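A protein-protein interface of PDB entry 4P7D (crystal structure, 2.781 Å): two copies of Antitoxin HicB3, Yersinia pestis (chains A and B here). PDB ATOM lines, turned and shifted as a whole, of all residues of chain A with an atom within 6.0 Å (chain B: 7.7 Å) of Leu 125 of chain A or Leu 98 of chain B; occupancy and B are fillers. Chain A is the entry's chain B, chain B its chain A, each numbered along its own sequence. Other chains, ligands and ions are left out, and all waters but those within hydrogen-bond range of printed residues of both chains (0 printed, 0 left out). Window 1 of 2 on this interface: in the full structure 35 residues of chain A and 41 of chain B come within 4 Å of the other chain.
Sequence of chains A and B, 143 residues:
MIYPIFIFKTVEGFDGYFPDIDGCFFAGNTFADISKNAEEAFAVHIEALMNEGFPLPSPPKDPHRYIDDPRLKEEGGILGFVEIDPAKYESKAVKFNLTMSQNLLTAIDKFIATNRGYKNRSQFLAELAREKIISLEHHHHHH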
ATOM      1  N   VAL A  94      14.849  26.978  -4.681  1.00  0.00           N
ATOM      2  CA  VAL A  94      13.942  26.259  -5.559  1.00  0.00           C
ATOM      3  C   VAL A  94      14.720  25.277  -6.406  1.00  0.00           C
ATOM      4  O   VAL A  94      15.724  25.655  -7.012  1.00  0.00           O
ATOM      5  CB  VAL A  94      13.152  27.194  -6.452  1.00  0.00           C
ATOM      6  CG1 VAL A  94      12.459  26.403  -7.551  1.00  0.00           C
ATOM      7  CG2 VAL A  94      12.134  27.949  -5.612  1.00  0.00           C
ATOM      8  N   LYS A  95      14.269  24.018  -6.412  1.00  0.00           N
ATOM      9  CA  LYS A  95      14.875  22.963  -7.227  1.00  0.00           C
ATOM     10  C   LYS A  95      14.017  22.712  -8.440  1.00  0.00           C
ATOM     11  O   LYS A  95      12.817  22.520  -8.310  1.00  0.00           O
ATOM     12  CB  LYS A  95      15.035  21.654  -6.448  1.00  0.00           C
ATOM     13  CG  LYS A  95      16.041  21.672  -5.338  1.00  0.00           C
ATOM     14  CD  LYS A  95      16.096  20.330  -4.635  1.00  0.00           C
ATOM     15  CE  LYS A  95      17.058  19.388  -5.298  1.00  0.00           C
ATOM     16  NZ  LYS A  95      18.454  19.903  -5.203  1.00  0.00           N
ATOM     17  N   PHE A  96      14.626  22.691  -9.616  1.00  0.00           N
ATOM     18  CA  PHE A  96      13.857  22.502 -10.835  1.00  0.00           C
ATOM     19  C   PHE A  96      14.625  21.792 -11.921  1.00  0.00           C
ATOM     20  O   PHE A  96      15.828  21.588 -11.828  1.00  0.00           O
ATOM     21  CB  PHE A  96      13.348  23.843 -11.379  1.00  0.00           C
ATOM     22  CG  PHE A  96      14.426  24.826 -11.665  1.00  0.00           C
ATOM     23  CD1 PHE A  96      15.059  25.521 -10.619  1.00  0.00           C
ATOM     24  CD2 PHE A  96      14.821  25.071 -12.966  1.00  0.00           C
ATOM     25  CE1 PHE A  96      16.075  26.442 -10.877  1.00  0.00           C
ATOM     26  CE2 PHE A  96      15.836  25.989 -13.227  1.00  0.00           C
ATOM     27  CZ  PHE A  96      16.463  26.676 -12.175  1.00  0.00           C
ATOM     28  N   ASN A  97      13.891  21.432 -12.964  1.00  0.00           N
ATOM     29  CA  ASN A  97      14.411  20.658 -14.066  1.00  0.00           C
ATOM     30  C   ASN A  97      14.608  21.472 -15.318  1.00  0.00           C
ATOM     31  O   ASN A  97      13.839  22.381 -15.624  1.00  0.00           O
ATOM     32  CB  ASN A  97      13.466  19.520 -14.359  1.00  0.00           C
ATOM     33  CG  ASN A  97      13.395  18.566 -13.241  1.00  0.00           C
ATOM     34  OD1 ASN A  97      14.404  18.274 -12.611  1.00  0.00           O
ATOM     35  ND2 ASN A  97      12.205  18.091 -12.947  1.00  0.00           N
ATOM     36  N   LEU A  98      15.651  21.110 -16.039  1.00  0.00           N
ATOM     37  CA  LEU A  98      15.959  21.646 -17.342  1.00  0.00           C
ATOM     38  C   LEU A  98      16.218  20.493 -18.299  1.00  0.00           C
ATOM     39  O   LEU A  98      16.453  19.354 -17.881  1.00  0.00           O
ATOM     40  CB  LEU A  98      17.179  22.552 -17.269  1.00  0.00           C
ATOM     41  CG  LEU A  98      17.144  23.637 -16.203  1.00  0.00           C
ATOM     42  CD1 LEU A  98      18.372  24.516 -16.358  1.00  0.00           C
ATOM     43  CD2 LEU A  98      15.905  24.475 -16.345  1.00  0.00           C
ATOM     44  N   MET A 100      18.774  20.035 -21.592  1.00  0.00           N
ATOM     45  CA  MET A 100      19.559  20.409 -22.748  1.00  0.00           C
ATOM     46  C   MET A 100      20.374  19.248 -23.312  1.00  0.00           C
ATOM     47  O   MET A 100      20.481  18.196 -22.699  1.00  0.00           O
ATOM     48  CB  MET A 100      20.436  21.625 -22.432  1.00  0.00           C
ATOM     49  CG  MET A 100      21.243  21.542 -21.188  1.00  0.00           C
ATOM     50  SD  MET A 100      22.250  23.193 -20.830  1.00  0.00           S
ATOM     51  CE  MET A 100      20.923  24.394 -20.072  1.00  0.00           C
ATOM     52  N   ILE A 108      29.671  22.105 -20.379  1.00  0.00           N
ATOM     53  CA  ILE A 108      29.579  22.896 -19.163  1.00  0.00           C
ATOM     54  C   ILE A 108      30.343  22.239 -18.020  1.00  0.00           C
ATOM     55  O   ILE A 108      31.106  22.892 -17.316  1.00  0.00           O
ATOM     56  CB  ILE A 108      28.122  23.122 -18.753  1.00  0.00           C
ATOM     57  CG1 ILE A 108      27.508  24.169 -19.668  1.00  0.00           C
ATOM     58  CG2 ILE A 108      28.045  23.597 -17.319  1.00  0.00           C
ATOM     59  CD1 ILE A 108      26.009  24.218 -19.609  1.00  0.00           C
ATOM     60  N   ASN A 120      29.621  24.067  -8.446  1.00  0.00           N
ATOM     61  CA  ASN A 120      28.758  23.169  -9.190  1.00  0.00           C
ATOM     62  C   ASN A 120      27.939  23.866 -10.287  1.00  0.00           C
ATOM     63  O   ASN A 120      28.155  25.039 -10.566  1.00  0.00           O
ATOM     64  CB  ASN A 120      27.847  22.454  -8.215  1.00  0.00           C
ATOM     65  CG  ASN A 120      27.211  23.391  -7.270  1.00  0.00           C
ATOM     66  OD1 ASN A 120      26.485  24.285  -7.683  1.00  0.00           O
ATOM     67  ND2 ASN A 120      27.492  23.229  -5.989  1.00  0.00           N
ATOM     68  N   ARG A 121      27.020  23.124 -10.914  1.00  0.00           N
ATOM     69  CA  ARG A 121      26.217  23.624 -12.019  1.00  0.00           C
ATOM     70  C   ARG A 121      25.246  24.696 -11.590  1.00  0.00           C
ATOM     71  O   ARG A 121      25.045  25.689 -12.293  1.00  0.00           O
ATOM     72  CB  ARG A 121      25.423  22.507 -12.671  1.00  0.00           C
ATOM     73  CG  ARG A 121      26.213  21.563 -13.535  1.00  0.00           C
ATOM     74  CD  ARG A 121      25.269  20.663 -14.324  1.00  0.00           C
ATOM     75  NE  ARG A 121      25.909  19.390 -14.646  1.00  0.00           N
ATOM     76  CZ  ARG A 121      25.357  18.207 -14.417  1.00  0.00           C
ATOM     77  NH1 ARG A 121      24.149  18.144 -13.878  1.00  0.00           N
ATOM     78  NH2 ARG A 121      26.007  17.098 -14.740  1.00  0.00           N
ATOM     79  N   SER A 122      24.610  24.498 -10.449  1.00  0.00           N
ATOM     80  CA  SER A 122      23.674  25.512  -9.992  1.00  0.00           C
ATOM     81  C   SER A 122      24.390  26.840  -9.720  1.00  0.00           C
ATOM     82  O   SER A 122      23.890  27.888 -10.088  1.00  0.00           O
ATOM     83  CB  SER A 122      22.920  25.028  -8.758  1.00  0.00           C
ATOM     84  OG  SER A 122      22.133  23.905  -9.100  1.00  0.00           O
ATOM     85  N   GLN A 123      25.569  26.808  -9.112  1.00  0.00           N
ATOM     86  CA  GLN A 123      26.257  28.060  -8.824  1.00  0.00           C
ATOM     87  C   GLN A 123      26.665  28.750 -10.114  1.00  0.00           C
ATOM     88  O   GLN A 123      26.494  29.972 -10.275  1.00  0.00           O
ATOM     89  CB  GLN A 123      27.493  27.840  -7.943  1.00  0.00           C
ATOM     90  CG  GLN A 123      28.012  29.144  -7.348  1.00  0.00           C
ATOM     91  CD  GLN A 123      29.351  28.984  -6.663  1.00  0.00           C
ATOM     92  OE1 GLN A 123      30.346  28.623  -7.297  1.00  0.00           O
ATOM     93  NE2 GLN A 123      29.383  29.237  -5.352  1.00  0.00           N
ATOM     94  N   PHE A 124      27.196  27.947 -11.032  1.00  0.00           N
ATOM     95  CA  PHE A 124      27.663  28.441 -12.321  1.00  0.00           C
ATOM     96  C   PHE A 124      26.549  29.090 -13.154  1.00  0.00           C
ATOM     97  O   PHE A 124      26.686  30.231 -13.604  1.00  0.00           O
ATOM     98  CB  PHE A 124      28.307  27.296 -13.090  1.00  0.00           C
ATOM     99  CG  PHE A 124      28.650  27.629 -14.505  1.00  0.00           C
ATOM    100  CD1 PHE A 124      29.786  28.339 -14.802  1.00  0.00           C
ATOM    101  CD2 PHE A 124      27.834  27.230 -15.534  1.00  0.00           C
ATOM    102  CE1 PHE A 124      30.109  28.635 -16.091  1.00  0.00           C
ATOM    103  CE2 PHE A 124      28.151  27.534 -16.825  1.00  0.00           C
ATOM    104  CZ  PHE A 124      29.290  28.234 -17.100  1.00  0.00           C
ATOM    105  N   LEU A 125      25.443  28.378 -13.359  1.00  0.00           N
ATOM    106  CA  LEU A 125      24.355  28.937 -14.170  1.00  0.00           C
ATOM    107  C   LEU A 125      23.596  30.020 -13.415  1.00  0.00           C
ATOM    108  O   LEU A 125      23.010  30.898 -14.056  1.00  0.00           O
ATOM    109  CB  LEU A 125      23.383  27.845 -14.633  1.00  0.00           C
ATOM    110  CG  LEU A 125      24.022  26.712 -15.436  1.00  0.00           C
ATOM    111  CD1 LEU A 125      23.196  25.495 -15.300  1.00  0.00           C
ATOM    112  CD2 LEU A 125      24.110  27.071 -16.888  1.00  0.00           C
ATOM    113  N   ALA A 126      23.596  29.971 -12.074  1.00  0.00           N
ATOM    114  CA  ALA A 126      22.987  31.059 -11.297  1.00  0.00           C
ATOM    115  C   ALA A 126      23.831  32.330 -11.454  1.00  0.00           C
ATOM    116  O   ALA A 126      23.303  33.403 -11.697  1.00  0.00           O
ATOM    117  CB  ALA A 126      22.851  30.699  -9.863  1.00  0.00           C
ATOM    118  N   GLU A 127      25.151  32.204 -11.345  1.00  0.00           N
ATOM    119  CA  GLU A 127      25.999  33.366 -11.526  1.00  0.00           C
ATOM    120  C   GLU A 127      25.796  33.977 -12.922  1.00  0.00           C
ATOM    121  O   GLU A 127      25.578  35.197 -13.029  1.00  0.00           O
ATOM    122  CB  GLU A 127      27.467  33.019 -11.261  1.00  0.00           C
ATOM    123  CG  GLU A 127      28.085  33.979 -10.273  1.00  0.00           C
ATOM    124  CD  GLU A 127      29.238  33.371  -9.490  1.00  0.00           C
ATOM    125  OE1 GLU A 127      30.360  33.232 -10.039  1.00  0.00           O
ATOM    126  OE2 GLU A 127      29.006  33.023  -8.305  1.00  0.00           O
ATOM    127  N   LEU A 128      25.839  33.154 -13.973  1.00  0.00           N
ATOM    128  CA  LEU A 128      25.612  33.666 -15.319  1.00  0.00           C
ATOM    129  C   LEU A 128      24.242  34.336 -15.463  1.00  0.00           C
ATOM    130  O   LEU A 128      24.071  35.239 -16.275  1.00  0.00           O
ATOM    131  CB  LEU A 128      25.723  32.555 -16.353  1.00  0.00           C
ATOM    132  CG  LEU A 128      27.045  31.862 -16.672  1.00  0.00           C
ATOM    133  CD1 LEU A 128      26.828  30.928 -17.808  1.00  0.00           C
ATOM    134  CD2 LEU A 128      28.147  32.829 -17.002  1.00  0.00           C
ATOM    135  N   ALA A 129      23.270  33.904 -14.675  1.00  0.00           N
ATOM    136  CA  ALA A 129      21.900  34.381 -14.855  1.00  0.00           C
ATOM    137  C   ALA A 129      21.665  35.698 -14.156  1.00  0.00           C
ATOM    138  O   ALA A 129      20.948  36.552 -14.662  1.00  0.00           O
ATOM    139  CB  ALA A 129      20.890  33.327 -14.354  1.00  0.00           C
ATOM    140  N   ARG A 130      22.263  35.865 -12.983  1.00  0.00           N
ATOM    141  CA  ARG A 130      22.067  37.092 -12.223  1.00  0.00           C
ATOM    142  C   ARG A 130      22.737  38.294 -12.897  1.00  0.00           C
ATOM    143  O   ARG A 130      22.279  39.417 -12.752  1.00  0.00           O
ATOM    144  CB  ARG A 130      22.584  36.912 -10.804  1.00  0.00           C
ATOM    145  CG  ARG A 130      22.365  38.090  -9.880  1.00  0.00           C
ATOM    146  CD  ARG A 130      23.067  37.838  -8.546  1.00  0.00           C
ATOM    147  NE  ARG A 130      22.551  36.691  -7.796  1.00  0.00           N
ATOM    148  CZ  ARG A 130      21.372  36.676  -7.176  1.00  0.00           C
ATOM    149  NH1 ARG A 130      20.575  37.736  -7.255  1.00  0.00           N
ATOM    150  NH2 ARG A 130      20.973  35.598  -6.503  1.00  0.00           N
ATOM    151  N   PHE B  96      18.146  17.421 -16.349  1.00  0.00           N
ATOM    152  CA  PHE B  96      18.901  17.555 -15.104  1.00  0.00           C
ATOM    153  C   PHE B  96      18.278  18.560 -14.148  1.00  0.00           C
ATOM    154  O   PHE B  96      17.241  19.138 -14.405  1.00  0.00           O
ATOM    155  CB  PHE B  96      20.365  17.901 -15.383  1.00  0.00           C
ATOM    156  CG  PHE B  96      20.570  19.188 -16.092  1.00  0.00           C
ATOM    157  CD1 PHE B  96      20.402  19.270 -17.478  1.00  0.00           C
ATOM    158  CD2 PHE B  96      21.008  20.322 -15.389  1.00  0.00           C
ATOM    159  CE1 PHE B  96      20.614  20.476 -18.142  1.00  0.00           C
ATOM    160  CE2 PHE B  96      21.224  21.537 -16.068  1.00  0.00           C
ATOM    161  CZ  PHE B  96      21.024  21.612 -17.427  1.00  0.00           C
ATOM    162  N   ASN B  97      18.901  18.739 -13.010  1.00  0.00           N
ATOM    163  CA  ASN B  97      18.242  19.437 -11.942  1.00  0.00           C
ATOM    164  C   ASN B  97      19.181  20.516 -11.414  1.00  0.00           C
ATOM    165  O   ASN B  97      20.397  20.322 -11.370  1.00  0.00           O
ATOM    166  CB  ASN B  97      17.830  18.420 -10.871  1.00  0.00           C
ATOM    167  CG  ASN B  97      16.814  18.961  -9.888  1.00  0.00           C
ATOM    168  OD1 ASN B  97      17.142  19.235  -8.739  1.00  0.00           O
ATOM    169  ND2 ASN B  97      15.579  19.093 -10.321  1.00  0.00           N
ATOM    170  N   LEU B  98      18.614  21.663 -11.050  1.00  0.00           N
ATOM    171  CA  LEU B  98      19.380  22.795 -10.551  1.00  0.00           C
ATOM    172  C   LEU B  98      18.658  23.382  -9.363  1.00  0.00           C
ATOM    173  O   LEU B  98      17.427  23.365  -9.322  1.00  0.00           O
ATOM    174  CB  LEU B  98      19.535  23.876 -11.603  1.00  0.00           C
ATOM    175  CG  LEU B  98      20.254  23.659 -12.922  1.00  0.00           C
ATOM    176  CD1 LEU B  98      20.356  25.018 -13.515  1.00  0.00           C
ATOM    177  CD2 LEU B  98      21.641  23.046 -12.775  1.00  0.00           C
ATOM    178  N   THR B  99      19.418  23.913  -8.408  1.00  0.00           N
ATOM    179  CA  THR B  99      18.824  24.595  -7.289  1.00  0.00           C
ATOM    180  C   THR B  99      19.213  26.048  -7.315  1.00  0.00           C
ATOM    181  O   THR B  99      20.387  26.371  -7.460  1.00  0.00           O
ATOM    182  CB  THR B  99      19.266  23.981  -5.966  1.00  0.00           C
ATOM    183  OG1 THR B  99      19.058  22.564  -6.007  1.00  0.00           O
ATOM    184  CG2 THR B  99      18.471  24.585  -4.810  1.00  0.00           C
ATOM    185  N   MET B 100      18.244  26.938  -7.183  1.00  0.00           N
ATOM    186  CA  MET B 100      18.592  28.306  -6.873  1.00  0.00           C
ATOM    187  C   MET B 100      17.459  29.064  -6.170  1.00  0.00           C
ATOM    188  O   MET B 100      16.361  28.542  -5.981  1.00  0.00           O
ATOM    189  CB  MET B 100      19.072  29.017  -8.141  1.00  0.00           C
ATOM    190  CG  MET B 100      18.108  29.072  -9.286  1.00  0.00           C
ATOM    191  SD  MET B 100      18.978  29.745 -10.961  1.00  0.00           S
ATOM    192  CE  MET B 100      19.745  28.113 -11.688  1.00  0.00           C
ATOM    193  N   LEU B 104      15.814  34.579  -7.814  1.00  0.00           N
ATOM    194  CA  LEU B 104      16.475  34.439  -9.103  1.00  0.00           C
ATOM    195  C   LEU B 104      15.576  33.703 -10.132  1.00  0.00           C
ATOM    196  O   LEU B 104      15.431  34.136 -11.285  1.00  0.00           O
ATOM    197  CB  LEU B 104      17.813  33.719  -8.933  1.00  0.00           C
ATOM    198  CG  LEU B 104      18.747  33.708 -10.145  1.00  0.00           C
ATOM    199  CD1 LEU B 104      18.793  35.107 -10.710  1.00  0.00           C
ATOM    200  CD2 LEU B 104      20.145  33.213  -9.774  1.00  0.00           C
ATOM    201  N   LEU B 105      14.946  32.610  -9.720  1.00  0.00           N
ATOM    202  CA  LEU B 105      14.110  31.866 -10.657  1.00  0.00           C
ATOM    203  C   LEU B 105      12.883  32.679 -11.096  1.00  0.00           C
ATOM    204  O   LEU B 105      12.417  32.528 -12.218  1.00  0.00           O
ATOM    205  CB  LEU B 105      13.671  30.523 -10.062  1.00  0.00           C
ATOM    206  CG  LEU B 105      13.050  29.563 -11.086  1.00  0.00           C
ATOM    207  CD1 LEU B 105      13.983  29.319 -12.247  1.00  0.00           C
ATOM    208  CD2 LEU B 105      12.681  28.241 -10.474  1.00  0.00           C
ATOM    209  N   ILE B 108      14.337  35.198 -13.817  1.00  0.00           N
ATOM    210  CA  ILE B 108      14.549  34.462 -15.059  1.00  0.00           C
ATOM    211  C   ILE B 108      13.223  34.260 -15.809  1.00  0.00           C
ATOM    212  O   ILE B 108      13.157  34.417 -17.024  1.00  0.00           O
ATOM    213  CB  ILE B 108      15.213  33.099 -14.781  1.00  0.00           C
ATOM    214  CG1 ILE B 108      16.615  33.313 -14.213  1.00  0.00           C
ATOM    215  CG2 ILE B 108      15.290  32.268 -16.026  1.00  0.00           C
ATOM    216  CD1 ILE B 108      17.273  32.052 -13.745  1.00  0.00           C
ATOM    217  N   SER B 122      15.240  26.405 -20.253  1.00  0.00           N
ATOM    218  CA  SER B 122      16.376  25.654 -20.756  1.00  0.00           C
ATOM    219  C   SER B 122      17.174  26.440 -21.785  1.00  0.00           C
ATOM    220  O   SER B 122      18.363  26.653 -21.606  1.00  0.00           O
ATOM    221  CB  SER B 122      15.910  24.296 -21.294  1.00  0.00           C
ATOM    222  OG  SER B 122      15.407  23.487 -20.216  1.00  0.00           O
ATOM    223  N   PHE B 124      17.240  29.614 -22.386  1.00  0.00           N
ATOM    224  CA  PHE B 124      17.819  30.822 -21.837  1.00  0.00           C
ATOM    225  C   PHE B 124      19.183  30.568 -21.173  1.00  0.00           C
ATOM    226  O   PHE B 124      20.212  31.175 -21.523  1.00  0.00           O
ATOM    227  CB  PHE B 124      16.843  31.406 -20.850  1.00  0.00           C
ATOM    228  CG  PHE B 124      17.382  32.561 -20.060  1.00  0.00           C
ATOM    229  CD1 PHE B 124      17.544  33.796 -20.647  1.00  0.00           C
ATOM    230  CD2 PHE B 124      17.669  32.422 -18.713  1.00  0.00           C
ATOM    231  CE1 PHE B 124      18.019  34.852 -19.928  1.00  0.00           C
ATOM    232  CE2 PHE B 124      18.124  33.473 -17.980  1.00  0.00           C
ATOM    233  CZ  PHE B 124      18.296  34.700 -18.580  1.00  0.00           C
ATOM    234  N   LEU B 125      19.179  29.643 -20.222  1.00  0.00           N
ATOM    235  CA  LEU B 125      20.395  29.230 -19.538  1.00  0.00           C
ATOM    236  C   LEU B 125      21.390  28.602 -20.518  1.00  0.00           C
ATOM    237  O   LEU B 125      22.612  28.747 -20.361  1.00  0.00           O
ATOM    238  CB  LEU B 125      20.050  28.269 -18.391  1.00  0.00           C
ATOM    239  CG  LEU B 125      19.153  28.944 -17.345  1.00  0.00           C
ATOM    240  CD1 LEU B 125      18.801  28.023 -16.219  1.00  0.00           C
ATOM    241  CD2 LEU B 125      19.855  30.162 -16.810  1.00  0.00           C
ATOM    242  N   ALA B 126      20.874  27.933 -21.549  1.00  0.00           N
ATOM    243  CA  ALA B 126      21.737  27.364 -22.586  1.00  0.00           C
ATOM    244  C   ALA B 126      22.445  28.445 -23.408  1.00  0.00           C
ATOM    245  O   ALA B 126      23.659  28.365 -23.603  1.00  0.00           O
ATOM    246  CB  ALA B 126      20.943  26.454 -23.490  1.00  0.00           C
ATOM    247  N   LEU B 128      22.976  31.383 -22.568  1.00  0.00           N
ATOM    248  CA  LEU B 128      23.835  32.013 -21.589  1.00  0.00           C
ATOM    249  C   LEU B 128      25.143  31.255 -21.342  1.00  0.00           C
ATOM    250  O   LEU B 128      26.226  31.849 -21.301  1.00  0.00           O
ATOM    251  CB  LEU B 128      23.068  32.156 -20.290  1.00  0.00           C
ATOM    252  CG  LEU B 128      23.033  33.517 -19.590  1.00  0.00           C
ATOM    253  CD1 LEU B 128      22.589  34.648 -20.509  1.00  0.00           C
ATOM    254  CD2 LEU B 128      22.109  33.420 -18.403  1.00  0.00           C
ATOM    255  N   ALA B 129      25.072  29.946 -21.163  1.00  0.00           N
ATOM    256  CA  ALA B 129      26.308  29.219 -20.911  1.00  0.00           C
ATOM    257  C   ALA B 129      27.203  29.173 -22.152  1.00  0.00           C
ATOM    258  O   ALA B 129      28.438  29.167 -22.034  1.00  0.00           O
ATOM    259  CB  ALA B 129      26.013  27.835 -20.434  1.00  0.00           C
ATOM    260  N   ARG B 130      26.582  29.145 -23.332  1.00  0.00           N
ATOM    261  CA  ARG B 130      27.326  29.106 -24.594  1.00  0.00           C
ATOM    262  C   ARG B 130      28.242  30.311 -24.734  1.00  0.00           C
ATOM    263  O   ARG B 130      29.421  30.159 -25.028  1.00  0.00           O
ATOM    264  CB  ARG B 130      26.382  29.056 -25.793  1.00  0.00           C
ATOM    265  CG  ARG B 130      25.969  27.674 -26.238  1.00  0.00           C
ATOM    266  CD  ARG B 130      24.974  27.750 -27.407  1.00  0.00           C
ATOM    267  NE  ARG B 130      24.283  26.474 -27.565  1.00  0.00           N
ATOM    268  CZ  ARG B 130      22.995  26.291 -27.307  1.00  0.00           C
ATOM    269  NH1 ARG B 130      22.239  27.318 -26.912  1.00  0.00           N
ATOM    270  NH2 ARG B 130      22.453  25.092 -27.468  1.00  0.00           N
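ND2 of Asn 97 of chain B is in hydrogen-bond range of O of Phe 96 of chain A, at 2.9 Å. N of Val 94 of chain A lies within hydrogen-bond range of O of Met 100 of chain B (2.5 Å). The side-chain hydroxyl of Thr 99 of chain B lies within hydrogen-bond range of the side-chain amino group of Lys 95 of chain A (2.8 Å). O of Phe 96 of chain A sits at hydrogen-bond distance from N of Leu 98 of chain B, at 2.9 Å. The side-chain amide oxygen (OD1) of Asn 97 of chain A lies close to the backbone carbonyl oxygen (O) of Phe 96 of chain B (3.5 Å). The side-chain amide nitrogen of Asn 97 of chain B is in hydrogen-bond range of the side-chain amide oxygen of Asn 97 of chain A (2.7 Å). The backbone NH of Thr 99 of chain B sits at hydrogen-bond distance from the side-chain hydroxyl of Ser 122 of chain A, 2.8 Å away. The backbone NH (N) of Phe 96 of chain B lies within hydrogen-bond range of the backbone carbonyl oxygen (O) of Leu 98 of chain A (3.0 Å).
The side-chain amide oxygen of Asn 120 of chain A is in hydrogen-bond range of the backbone NH of Ser 122 of chain A.
Among the printed residues, pairs that only touch across the chains: Met 100 of chain A with Phe 96 of chain B (3.3 Å), Val 94 of chain A with Thr 99 of chain B (3.3 Å), Ser 122 of chain A with Leu 98 of chain B (3.3 Å), Lys 95 of chain A with Leu 98 of chain B (3.3 Å), Leu 125 of chain A with Leu 98 of chain B (3.4 Å), Leu 128 of chain A with Leu 128 of chain B (3.4 Å), Lys 95 of chain A with Asn 97 of chain B (3.4 Å), Leu 98 of chain A with Ser 122 of chain B (3.5 Å), Val 94 of chain A with Leu 105 of chain B (3.5 Å), Leu 98 of chain A with Leu 98 of chain B (3.5 Å), Leu 98 of chain A with Leu 125 of chain B (3.5 Å), Leu 128 of chain A with Ala 129 of chain B (3.6 Å), Phe 96 of chain A with Met 100 of chain B (3.6 Å), Phe 96 of chain A with Leu 105 of chain B (3.6 Å), Val 94 of chain A with Leu 98 of chain B (3.7 Å), Ala 129 of chain A with Leu 128 of chain B (3.7 Å), Ala 126 of chain A with Leu 104 of chain B (3.7 Å), Ile 108 of chain A with Ala 129 of chain B (3.7 Å), Met 100 of chain A with Ser 122 of chain B (3.7 Å), Arg 121 of chain A with Leu 98 of chain B (3.8 Å), Phe 96 of chain A with Phe 96 of chain B (3.8 Å), Met 100 of chain A with Ala 126 of chain B (3.8 Å) and Ala 129 of chain A with Ile 108 of chain B (3.9 Å).
Of the printed residues of chain B, Val 94 of chain A touches Leu 98, Thr 99, Met 100 and Leu 105. Printed residues of chain B within 4 Å of Arg 121 of chain A: Leu 98. Leu 125 of chain A touches just one residue of chain B: Leu 98 (3.4 Å). Printed residues of chain A within 4 Å of Thr 99 of chain B: Val 94 (3.3 Å), Lys 95 (2.8 Å) and Ser 122 (2.8 Å). Printed residues of chain A within 4 Å of Leu 104 of chain B: Ala 126 (3.7 Å). The nearest printed residue of chain B that does not touch Ala 129 of chain A is Leu 125 of chain B (4.1 Å).
Of the 15 printed residues of chain B, 13 touch a printed residue of chain A. Hydrophobic or aromatic side chains of chain B within 4 Å of the printed part of chain A: Phe 96, Leu 98, Met 100, Leu 104, Leu 105, Ile 108, Leu 125, Ala 126, Leu 128 and Ala 129. Hydrophobic or aromatic side chains of chain A within 4 Å of the printed part of chain B: Val 94, Phe 96, Leu 98, Met 100, Ile 108, Leu 125, Ala 126, Leu 128 and Ala 129. Among the printed residues, 31 pairs touch across the chains.
Phe 96 of chain A touches Asn 97 of chain B, and with the chains exchanged Asn 97 of chain A touches Phe 96 of chain B. Leu 98 of chain B touches its own counterpart, Leu 98 of chain A. Ile 108 of chain A touches Ala 129 of chain B, and with the chains exchanged Ala 129 of chain A touches Ile 108 of chain B. Leu 128 of chain A touches Ala 129 of chain B, and with the chains exchanged Ala 129 of chain A touches Leu 128 of chain B.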
